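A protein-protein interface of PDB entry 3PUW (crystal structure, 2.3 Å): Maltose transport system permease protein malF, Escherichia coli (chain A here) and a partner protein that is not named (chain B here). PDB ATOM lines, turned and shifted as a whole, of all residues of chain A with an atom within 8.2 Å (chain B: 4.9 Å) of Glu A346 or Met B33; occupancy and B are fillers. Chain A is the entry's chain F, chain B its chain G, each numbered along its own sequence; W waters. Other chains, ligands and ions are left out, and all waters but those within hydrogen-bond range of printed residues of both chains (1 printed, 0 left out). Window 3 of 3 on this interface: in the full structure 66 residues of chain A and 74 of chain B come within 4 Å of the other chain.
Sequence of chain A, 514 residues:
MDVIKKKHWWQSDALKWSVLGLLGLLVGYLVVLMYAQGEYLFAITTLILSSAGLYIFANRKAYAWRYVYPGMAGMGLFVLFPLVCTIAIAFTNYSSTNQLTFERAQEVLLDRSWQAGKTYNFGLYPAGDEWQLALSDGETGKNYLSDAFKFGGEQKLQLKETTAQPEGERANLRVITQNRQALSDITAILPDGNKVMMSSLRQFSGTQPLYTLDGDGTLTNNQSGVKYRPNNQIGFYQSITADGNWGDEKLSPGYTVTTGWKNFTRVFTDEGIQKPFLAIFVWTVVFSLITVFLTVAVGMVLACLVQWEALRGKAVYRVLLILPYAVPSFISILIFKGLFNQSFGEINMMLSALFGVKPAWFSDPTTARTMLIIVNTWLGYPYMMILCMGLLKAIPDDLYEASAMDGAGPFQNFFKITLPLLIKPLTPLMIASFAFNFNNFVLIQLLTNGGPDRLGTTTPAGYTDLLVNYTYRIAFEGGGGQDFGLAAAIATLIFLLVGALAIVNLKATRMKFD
The backbone NH (N) of Ile A347 sits close to the backbone carbonyl oxygen (O) of Leu A339 (3.4 Å).
CD1 of Ile A331 touches CG1 of Val B34, at 3.9 Å. Ile A335 touches Pro B30. CD1 of Ile A335 touches C of Met B33 (3.7 Å). Val B34 touches Ile A335. Ile A335 touches Ile B37. Pro B30 touches Phe A336 (CG to CZ, 3.5 Å). Phe B29 touches Leu A339 (CE2 to CD2, 3.8 Å). CG of Glu A346 touches CE2 of Phe B29, 3.7 Å away. Met B33 touches Glu A346 (CE to OE1, 3.6 Å).
Printed residues of chain B within 4 Å of Ile A331: Val B34. Printed residues of chain B within 4 Å of Ile A335: Pro B30, Met B33, Val B34 and Ile B37. Printed residues of chain B within 4 Å of Leu A339: Phe B29. Phe A344 touches none of the printed residues of chain B. Of chain B, only Phe B29 and Met B33 come within 4 Å of Glu A346. Met B33 touches just these residues of chain A: Ile A335 and Glu A346. Printed residues of chain A within 4 Å of Val B34: Ile A331 and Ile A335. Of the printed residues of chain A, Ile B37 touches Ile A335 (3.6 Å).
Printed residues of chain A that touch a printed residue of chain B: Ile A331, Ile A335, Phe A336, Leu A339 and Glu A346. Of the 11 printed residues of chain B, 5 touch a printed residue of chain A. Printed residues of chain B that touch a printed residue of chain A: Phe B29, Pro B30, Met B33, Val B34 and Ile B37. Among the printed residues, no Asp or Glu carboxylate lies within 4 Å of a Lys or Arg side-chain nitrogen of the other chain.
Water W1 bridges OE1 of Glu A346 (3.1 Å) and N of Gly B47 (3.4 Å).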
ATOM      1  N   ILE A 331      27.236 -34.971  -7.682  1.00  0.00           N
ATOM      2  CA  ILE A 331      27.066 -33.528  -7.853  1.00  0.00           C
ATOM      3  C   ILE A 331      26.361 -33.190  -9.172  1.00  0.00           C
ATOM      4  O   ILE A 331      25.447 -32.359  -9.193  1.00  0.00           O
ATOM      5  CB  ILE A 331      28.405 -32.746  -7.713  1.00  0.00           C
ATOM      6  CG1 ILE A 331      28.132 -31.243  -7.552  1.00  0.00           C
ATOM      7  CG2 ILE A 331      29.346 -33.029  -8.885  1.00  0.00           C
ATOM      8  CD1 ILE A 331      29.287 -30.452  -6.979  1.00  0.00           C
ATOM      9  N   ILE A 335      23.106 -30.912  -9.842  1.00  0.00           N
ATOM     10  CA  ILE A 335      23.213 -29.751 -10.719  1.00  0.00           C
ATOM     11  C   ILE A 335      22.197 -29.799 -11.872  1.00  0.00           C
ATOM     12  O   ILE A 335      21.574 -28.780 -12.192  1.00  0.00           O
ATOM     13  CB  ILE A 335      24.666 -29.526 -11.193  1.00  0.00           C
ATOM     14  CG1 ILE A 335      25.362 -28.592 -10.203  1.00  0.00           C
ATOM     15  CG2 ILE A 335      24.720 -28.960 -12.615  1.00  0.00           C
ATOM     16  CD1 ILE A 335      26.703 -28.096 -10.659  1.00  0.00           C
ATOM     17  N   PHE A 336      22.015 -30.980 -12.465  1.00  0.00           N
ATOM     18  CA  PHE A 336      20.958 -31.188 -13.458  1.00  0.00           C
ATOM     19  C   PHE A 336      19.576 -30.873 -12.874  1.00  0.00           C
ATOM     20  O   PHE A 336      18.734 -30.278 -13.549  1.00  0.00           O
ATOM     21  CB  PHE A 336      20.984 -32.615 -14.027  1.00  0.00           C
ATOM     22  CG  PHE A 336      21.818 -32.769 -15.284  1.00  0.00           C
ATOM     23  CD1 PHE A 336      22.950 -33.579 -15.288  1.00  0.00           C
ATOM     24  CD2 PHE A 336      21.463 -32.118 -16.462  1.00  0.00           C
ATOM     25  CE1 PHE A 336      23.725 -33.731 -16.447  1.00  0.00           C
ATOM     26  CE2 PHE A 336      22.232 -32.261 -17.620  1.00  0.00           C
ATOM     27  CZ  PHE A 336      23.364 -33.073 -17.612  1.00  0.00           C
ATOM     28  N   LYS A 337      19.358 -31.269 -11.620  1.00  0.00           N
ATOM     29  CA  LYS A 337      18.125 -30.960 -10.900  1.00  0.00           C
ATOM     30  C   LYS A 337      17.911 -29.448 -10.811  1.00  0.00           C
ATOM     31  O   LYS A 337      16.784 -28.961 -10.944  1.00  0.00           O
ATOM     32  CB  LYS A 337      18.156 -31.582  -9.506  1.00  0.00           C
ATOM     33  CG  LYS A 337      16.807 -31.649  -8.814  1.00  0.00           C
ATOM     34  CD  LYS A 337      16.982 -31.944  -7.330  1.00  0.00           C
ATOM     35  CE  LYS A 337      15.676 -31.776  -6.571  1.00  0.00           C
ATOM     36  NZ  LYS A 337      15.921 -31.473  -5.132  1.00  0.00           N
ATOM     37  N   GLY A 338      18.999 -28.713 -10.593  1.00  0.00           N
ATOM     38  CA  GLY A 338      18.971 -27.256 -10.640  1.00  0.00           C
ATOM     39  C   GLY A 338      18.665 -26.740 -12.035  1.00  0.00           C
ATOM     40  O   GLY A 338      17.782 -25.904 -12.205  1.00  0.00           O
ATOM     41  N   LEU A 339      19.385 -27.254 -13.033  1.00  0.00           N
ATOM     42  CA  LEU A 339      19.241 -26.805 -14.424  1.00  0.00           C
ATOM     43  C   LEU A 339      17.842 -27.041 -14.998  1.00  0.00           C
ATOM     44  O   LEU A 339      17.379 -26.279 -15.852  1.00  0.00           O
ATOM     45  CB  LEU A 339      20.279 -27.478 -15.335  1.00  0.00           C
ATOM     46  CG  LEU A 339      21.785 -27.326 -15.091  1.00  0.00           C
ATOM     47  CD1 LEU A 339      22.557 -28.063 -16.175  1.00  0.00           C
ATOM     48  CD2 LEU A 339      22.235 -25.873 -15.008  1.00  0.00           C
ATOM     49  N   PHE A 340      17.185 -28.100 -14.529  1.00  0.00           N
ATOM     50  CA  PHE A 340      15.869 -28.496 -15.028  1.00  0.00           C
ATOM     51  C   PHE A 340      14.682 -27.906 -14.256  1.00  0.00           C
ATOM     52  O   PHE A 340      13.530 -28.215 -14.574  1.00  0.00           O
ATOM     53  CB  PHE A 340      15.753 -30.022 -15.089  1.00  0.00           C
ATOM     54  CG  PHE A 340      16.301 -30.630 -16.360  1.00  0.00           C
ATOM     55  CD1 PHE A 340      15.635 -30.461 -17.573  1.00  0.00           C
ATOM     56  CD2 PHE A 340      17.472 -31.381 -16.342  1.00  0.00           C
ATOM     57  CE1 PHE A 340      16.129 -31.024 -18.751  1.00  0.00           C
ATOM     58  CE2 PHE A 340      17.978 -31.951 -17.517  1.00  0.00           C
ATOM     59  CZ  PHE A 340      17.303 -31.772 -18.722  1.00  0.00           C
ATOM     60  N   ASN A 341      14.951 -27.060 -13.260  1.00  0.00           N
ATOM     61  CA  ASN A 341      13.872 -26.394 -12.514  1.00  0.00           C
ATOM     62  C   ASN A 341      12.911 -25.701 -13.478  1.00  0.00           C
ATOM     63  O   ASN A 341      13.337 -25.001 -14.395  1.00  0.00           O
ATOM     64  CB  ASN A 341      14.424 -25.406 -11.476  1.00  0.00           C
ATOM     65  CG  ASN A 341      13.332 -24.827 -10.570  1.00  0.00           C
ATOM     66  OD1 ASN A 341      12.572 -23.941 -10.970  1.00  0.00           O
ATOM     67  ND2 ASN A 341      13.265 -25.323  -9.339  1.00  0.00           N
ATOM     68  N   GLN A 342      11.617 -25.925 -13.276  1.00  0.00           N
ATOM     69  CA  GLN A 342      10.597 -25.468 -14.218  1.00  0.00           C
ATOM     70  C   GLN A 342      10.516 -23.949 -14.379  1.00  0.00           C
ATOM     71  O   GLN A 342      10.387 -23.452 -15.501  1.00  0.00           O
ATOM     72  CB  GLN A 342       9.231 -26.052 -13.848  1.00  0.00           C
ATOM     73  CG  GLN A 342       9.160 -27.566 -14.011  1.00  0.00           C
ATOM     74  CD  GLN A 342       7.897 -28.181 -13.439  1.00  0.00           C
ATOM     75  OE1 GLN A 342       7.742 -29.402 -13.439  1.00  0.00           O
ATOM     76  NE2 GLN A 342       6.987 -27.342 -12.949  1.00  0.00           N
ATOM     77  N   SER A 343      10.601 -23.216 -13.269  1.00  0.00           N
ATOM     78  CA  SER A 343      10.500 -21.752 -13.304  1.00  0.00           C
ATOM     79  C   SER A 343      11.874 -21.092 -13.316  1.00  0.00           C
ATOM     80  O   SER A 343      12.077 -20.057 -13.960  1.00  0.00           O
ATOM     81  CB  SER A 343       9.691 -21.243 -12.117  1.00  0.00           C
ATOM     82  OG  SER A 343       8.606 -22.111 -11.857  1.00  0.00           O
ATOM     83  N   PHE A 344      12.804 -21.697 -12.587  1.00  0.00           N
ATOM     84  CA  PHE A 344      14.178 -21.240 -12.528  1.00  0.00           C
ATOM     85  C   PHE A 344      15.010 -22.268 -13.294  1.00  0.00           C
ATOM     86  O   PHE A 344      14.453 -23.077 -14.039  1.00  0.00           O
ATOM     87  CB  PHE A 344      14.612 -21.097 -11.064  1.00  0.00           C
ATOM     88  CG  PHE A 344      13.611 -20.352 -10.203  1.00  0.00           C
ATOM     89  CD1 PHE A 344      13.642 -18.962 -10.115  1.00  0.00           C
ATOM     90  CD2 PHE A 344      12.633 -21.043  -9.484  1.00  0.00           C
ATOM     91  CE1 PHE A 344      12.711 -18.271  -9.326  1.00  0.00           C
ATOM     92  CE2 PHE A 344      11.699 -20.361  -8.695  1.00  0.00           C
ATOM     93  CZ  PHE A 344      11.742 -18.975  -8.615  1.00  0.00           C
ATOM     94  N   GLY A 345      16.328 -22.253 -13.149  1.00  0.00           N
ATOM     95  CA  GLY A 345      17.148 -23.216 -13.886  1.00  0.00           C
ATOM     96  C   GLY A 345      17.340 -22.789 -15.327  1.00  0.00           C
ATOM     97  O   GLY A 345      16.376 -22.521 -16.048  1.00  0.00           O
ATOM     98  N   GLU A 346      18.600 -22.752 -15.744  1.00  0.00           N
ATOM     99  CA  GLU A 346      19.001 -22.074 -16.975  1.00  0.00           C
ATOM    100  C   GLU A 346      18.517 -22.694 -18.291  1.00  0.00           C
ATOM    101  O   GLU A 346      18.528 -22.019 -19.325  1.00  0.00           O
ATOM    102  CB  GLU A 346      20.513 -21.776 -16.989  1.00  0.00           C
ATOM    103  CG  GLU A 346      21.363 -22.619 -16.041  1.00  0.00           C
ATOM    104  CD  GLU A 346      21.180 -22.255 -14.570  1.00  0.00           C
ATOM    105  OE1 GLU A 346      21.701 -21.207 -14.137  1.00  0.00           O
ATOM    106  OE2 GLU A 346      20.525 -23.031 -13.842  1.00  0.00           O
ATOM    107  N   ILE A 347      18.075 -23.955 -18.249  1.00  0.00           N
ATOM    108  CA  ILE A 347      17.491 -24.616 -19.428  1.00  0.00           C
ATOM    109  C   ILE A 347      16.176 -23.950 -19.864  1.00  0.00           C
ATOM    110  O   ILE A 347      16.058 -23.516 -21.010  1.00  0.00           O
ATOM    111  CB  ILE A 347      17.334 -26.163 -19.244  1.00  0.00           C
ATOM    112  CG1 ILE A 347      18.683 -26.865 -19.454  1.00  0.00           C
ATOM    113  CG2 ILE A 347      16.295 -26.745 -20.212  1.00  0.00           C
ATOM    114  CD1 ILE A 347      18.711 -28.339 -19.056  1.00  0.00           C
ATOM    115  N   ASN A 348      15.210 -23.854 -18.952  1.00  0.00           N
ATOM    116  CA  ASN A 348      13.919 -23.241 -19.272  1.00  0.00           C
ATOM    117  C   ASN A 348      13.963 -21.718 -19.396  1.00  0.00           C
ATOM    118  O   ASN A 348      13.034 -21.117 -19.936  1.00  0.00           O
ATOM    119  CB  ASN A 348      12.827 -23.679 -18.286  1.00  0.00           C
ATOM    120  CG  ASN A 348      12.264 -25.061 -18.606  1.00  0.00           C
ATOM    121  OD1 ASN A 348      12.789 -25.779 -19.459  1.00  0.00           O
ATOM    122  ND2 ASN A 348      11.189 -25.434 -17.921  1.00  0.00           N
ATOM    123  N   MET A 349      15.035 -21.100 -18.899  1.00  0.00           N
ATOM    124  CA  MET A 349      15.266 -19.667 -19.110  1.00  0.00           C
ATOM    125  C   MET A 349      15.706 -19.417 -20.553  1.00  0.00           C
ATOM    126  O   MET A 349      15.455 -18.347 -21.113  1.00  0.00           O
ATOM    127  CB  MET A 349      16.310 -19.108 -18.132  1.00  0.00           C
ATOM    128  CG  MET A 349      15.920 -19.154 -16.648  1.00  0.00           C
ATOM    129  SD  MET A 349      14.593 -18.029 -16.141  1.00  0.00           S
ATOM    130  CE  MET A 349      15.432 -16.440 -16.133  1.00  0.00           C
ATOM    131  N   MET A 350      16.364 -20.418 -21.138  1.00  0.00           N
ATOM    132  CA  MET A 350      16.778 -20.398 -22.541  1.00  0.00           C
ATOM    133  C   MET A 350      15.635 -20.828 -23.473  1.00  0.00           C
ATOM    134  O   MET A 350      15.487 -20.292 -24.574  1.00  0.00           O
ATOM    135  CB  MET A 350      18.005 -21.295 -22.735  1.00  0.00           C
ATOM    136  CG  MET A 350      18.416 -21.521 -24.184  1.00  0.00           C
ATOM    137  SD  MET A 350      19.691 -22.780 -24.379  1.00  0.00           S
ATOM    138  CE  MET A 350      18.825 -24.283 -23.912  1.00  0.00           C
ATOM    139  N   LEU A 351      14.839 -21.798 -23.023  1.00  0.00           N
ATOM    140  CA  LEU A 351      13.648 -22.253 -23.749  1.00  0.00           C
ATOM    141  C   LEU A 351      12.488 -21.254 -23.642  1.00  0.00           C
ATOM    142  O   LEU A 351      11.460 -21.408 -24.305  1.00  0.00           O
ATOM    143  CB  LEU A 351      13.210 -23.638 -23.251  1.00  0.00           C
ATOM    144  CG  LEU A 351      13.726 -24.917 -23.922  1.00  0.00           C
ATOM    145  CD1 LEU A 351      15.240 -25.047 -23.868  1.00  0.00           C
ATOM    146  CD2 LEU A 351      13.082 -26.133 -23.285  1.00  0.00           C
ATOM    147  N   SER A 352      12.660 -20.236 -22.801  1.00  0.00           N
ATOM    148  CA  SER A 352      11.705 -19.135 -22.702  1.00  0.00           C
ATOM    149  C   SER A 352      12.015 -18.073 -23.755  1.00  0.00           C
ATOM    150  O   SER A 352      11.107 -17.549 -24.401  1.00  0.00           O
ATOM    151  CB  SER A 352      11.740 -18.517 -21.301  1.00  0.00           C
ATOM    152  OG  SER A 352      10.733 -17.530 -21.144  1.00  0.00           O
ATOM    153  N   ALA A 353      13.303 -17.768 -23.918  1.00  0.00           N
ATOM    154  CA  ALA A 353      13.769 -16.768 -24.878  1.00  0.00           C
ATOM    155  C   ALA A 353      13.637 -17.276 -26.312  1.00  0.00           C
ATOM    156  O   ALA A 353      13.048 -16.609 -27.165  1.00  0.00           O
ATOM    157  CB  ALA A 353      15.211 -16.373 -24.577  1.00  0.00           C
ATOM    158  N   PHE B  29      28.436 -27.864 -20.143  1.00  0.00           N
ATOM    159  CA  PHE B  29      27.716 -26.864 -19.355  1.00  0.00           C
ATOM    160  C   PHE B  29      27.492 -27.267 -17.890  1.00  0.00           C
ATOM    161  O   PHE B  29      27.830 -26.492 -16.994  1.00  0.00           O
ATOM    162  CB  PHE B  29      26.405 -26.434 -20.034  1.00  0.00           C
ATOM    163  CG  PHE B  29      25.759 -25.228 -19.395  1.00  0.00           C
ATOM    164  CD1 PHE B  29      26.261 -23.949 -19.627  1.00  0.00           C
ATOM    165  CD2 PHE B  29      24.656 -25.373 -18.559  1.00  0.00           C
ATOM    166  CE1 PHE B  29      25.672 -22.831 -19.033  1.00  0.00           C
ATOM    167  CE2 PHE B  29      24.060 -24.258 -17.963  1.00  0.00           C
ATOM    168  CZ  PHE B  29      24.570 -22.988 -18.200  1.00  0.00           C
ATOM    169  N   PRO B  30      26.954 -28.481 -17.637  1.00  0.00           N
ATOM    170  CA  PRO B  30      26.766 -28.884 -16.239  1.00  0.00           C
ATOM    171  C   PRO B  30      28.079 -28.897 -15.452  1.00  0.00           C
ATOM    172  O   PRO B  30      28.090 -28.555 -14.270  1.00  0.00           O
ATOM    173  CB  PRO B  30      26.211 -30.308 -16.358  1.00  0.00           C
ATOM    174  CG  PRO B  30      25.595 -30.359 -17.706  1.00  0.00           C
ATOM    175  CD  PRO B  30      26.471 -29.518 -18.568  1.00  0.00           C
ATOM    176  N   LEU B  31      29.171 -29.277 -16.113  1.00  0.00           N
ATOM    177  CA  LEU B  31      30.482 -29.355 -15.465  1.00  0.00           C
ATOM    178  C   LEU B  31      31.104 -27.992 -15.190  1.00  0.00           C
ATOM    179  O   LEU B  31      31.838 -27.828 -14.213  1.00  0.00           O
ATOM    180  CB  LEU B  31      31.447 -30.203 -16.292  1.00  0.00           C
ATOM    181  CG  LEU B  31      30.987 -31.626 -16.607  1.00  0.00           C
ATOM    182  CD1 LEU B  31      31.965 -32.278 -17.571  1.00  0.00           C
ATOM    183  CD2 LEU B  31      30.801 -32.457 -15.325  1.00  0.00           C
ATOM    184  N   LEU B  32      30.826 -27.026 -16.063  1.00  0.00           N
ATOM    185  CA  LEU B  32      31.279 -25.657 -15.860  1.00  0.00           C
ATOM    186  C   LEU B  32      30.543 -25.030 -14.681  1.00  0.00           C
ATOM    187  O   LEU B  32      31.100 -24.196 -13.961  1.00  0.00           O
ATOM    188  CB  LEU B  32      31.087 -24.820 -17.127  1.00  0.00           C
ATOM    189  CG  LEU B  32      31.962 -25.152 -18.343  1.00  0.00           C
ATOM    190  CD1 LEU B  32      31.451 -24.424 -19.582  1.00  0.00           C
ATOM    191  CD2 LEU B  32      33.443 -24.836 -18.101  1.00  0.00           C
ATOM    192  N   MET B  33      29.295 -25.449 -14.480  1.00  0.00           N
ATOM    193  CA  MET B  33      28.510 -25.013 -13.326  1.00  0.00           C
ATOM    194  C   MET B  33      29.081 -25.576 -12.021  1.00  0.00           C
ATOM    195  O   MET B  33      28.975 -24.946 -10.967  1.00  0.00           O
ATOM    196  CB  MET B  33      27.032 -25.385 -13.492  1.00  0.00           C
ATOM    197  CG  MET B  33      26.334 -24.703 -14.669  1.00  0.00           C
ATOM    198  SD  MET B  33      26.375 -22.889 -14.623  1.00  0.00           S
ATOM    199  CE  MET B  33      25.016 -22.522 -13.512  1.00  0.00           C
ATOM    200  N   VAL B  34      29.692 -26.756 -12.103  1.00  0.00           N
ATOM    201  CA  VAL B  34      30.401 -27.346 -10.968  1.00  0.00           C
ATOM    202  C   VAL B  34      31.667 -26.536 -10.677  1.00  0.00           C
ATOM    203  O   VAL B  34      31.958 -26.227  -9.519  1.00  0.00           O
ATOM    204  CB  VAL B  34      30.743 -28.842 -11.200  1.00  0.00           C
ATOM    205  CG1 VAL B  34      31.471 -29.433  -9.998  1.00  0.00           C
ATOM    206  CG2 VAL B  34      29.488 -29.647 -11.479  1.00  0.00           C
ATOM    207  N   VAL B  35      32.400 -26.186 -11.733  1.00  0.00           N
ATOM    208  CA  VAL B  35      33.589 -25.332 -11.630  1.00  0.00           C
ATOM    209  C   VAL B  35      33.227 -23.976 -11.020  1.00  0.00           C
ATOM    210  O   VAL B  35      33.955 -23.461 -10.171  1.00  0.00           O
ATOM    211  CB  VAL B  35      34.285 -25.148 -13.013  1.00  0.00           C
ATOM    212  CG1 VAL B  35      35.391 -24.100 -12.950  1.00  0.00           C
ATOM    213  CG2 VAL B  35      34.847 -26.482 -13.518  1.00  0.00           C
ATOM    214  N   ALA B  36      32.094 -23.417 -11.444  1.00  0.00           N
ATOM    215  CA  ALA B  36      31.582 -22.152 -10.911  1.00  0.00           C
ATOM    216  C   ALA B  36      31.298 -22.205  -9.407  1.00  0.00           C
ATOM    217  O   ALA B  36      31.582 -21.241  -8.688  1.00  0.00           O
ATOM    218  CB  ALA B  36      30.335 -21.724 -11.667  1.00  0.00           C
ATOM    219  N   ILE B  37      30.736 -23.321  -8.939  1.00  0.00           N
ATOM    220  CA  ILE B  37      30.444 -23.505  -7.515  1.00  0.00           C
ATOM    221  C   ILE B  37      31.742 -23.473  -6.711  1.00  0.00           C
ATOM    222  O   ILE B  37      31.805 -22.850  -5.652  1.00  0.00           O
ATOM    223  CB  ILE B  37      29.673 -24.822  -7.243  1.00  0.00           C
ATOM    224  CG1 ILE B  37      28.262 -24.747  -7.825  1.00  0.00           C
ATOM    225  CG2 ILE B  37      29.581 -25.109  -5.752  1.00  0.00           C
ATOM    226  CD1 ILE B  37      27.544 -26.076  -7.850  1.00  0.00           C
ATOM    227  N   GLY B  47      23.697 -20.141  -9.174  1.00  0.00           N
ATOM    228  CA  GLY B  47      24.260 -18.818  -9.423  1.00  0.00           C
ATOM    229  C   GLY B  47      24.699 -18.677 -10.866  1.00  0.00           C
ATOM    230  O   GLY B  47      24.444 -19.559 -11.691  1.00  0.00           O
ATOM    231  N   LEU B  49      27.205 -18.430 -14.163  1.00  0.00           N
ATOM    232  CA  LEU B  49      28.358 -19.167 -14.688  1.00  0.00           C
ATOM    233  C   LEU B  49      29.686 -18.523 -14.289  1.00  0.00           C
ATOM    234  O   LEU B  49      30.628 -19.217 -13.899  1.00  0.00           O
ATOM    235  CB  LEU B  49      28.260 -19.306 -16.215  1.00  0.00           C
ATOM    236  CG  LEU B  49      29.339 -20.113 -16.947  1.00  0.00           C
ATOM    237  CD1 LEU B  49      29.405 -21.538 -16.422  1.00  0.00           C
ATOM    238  CD2 LEU B  49      29.099 -20.109 -18.452  1.00  0.00           C
HETATM  239  O   HOH W   1      22.373 -22.432 -11.365  1.00  0.00           O
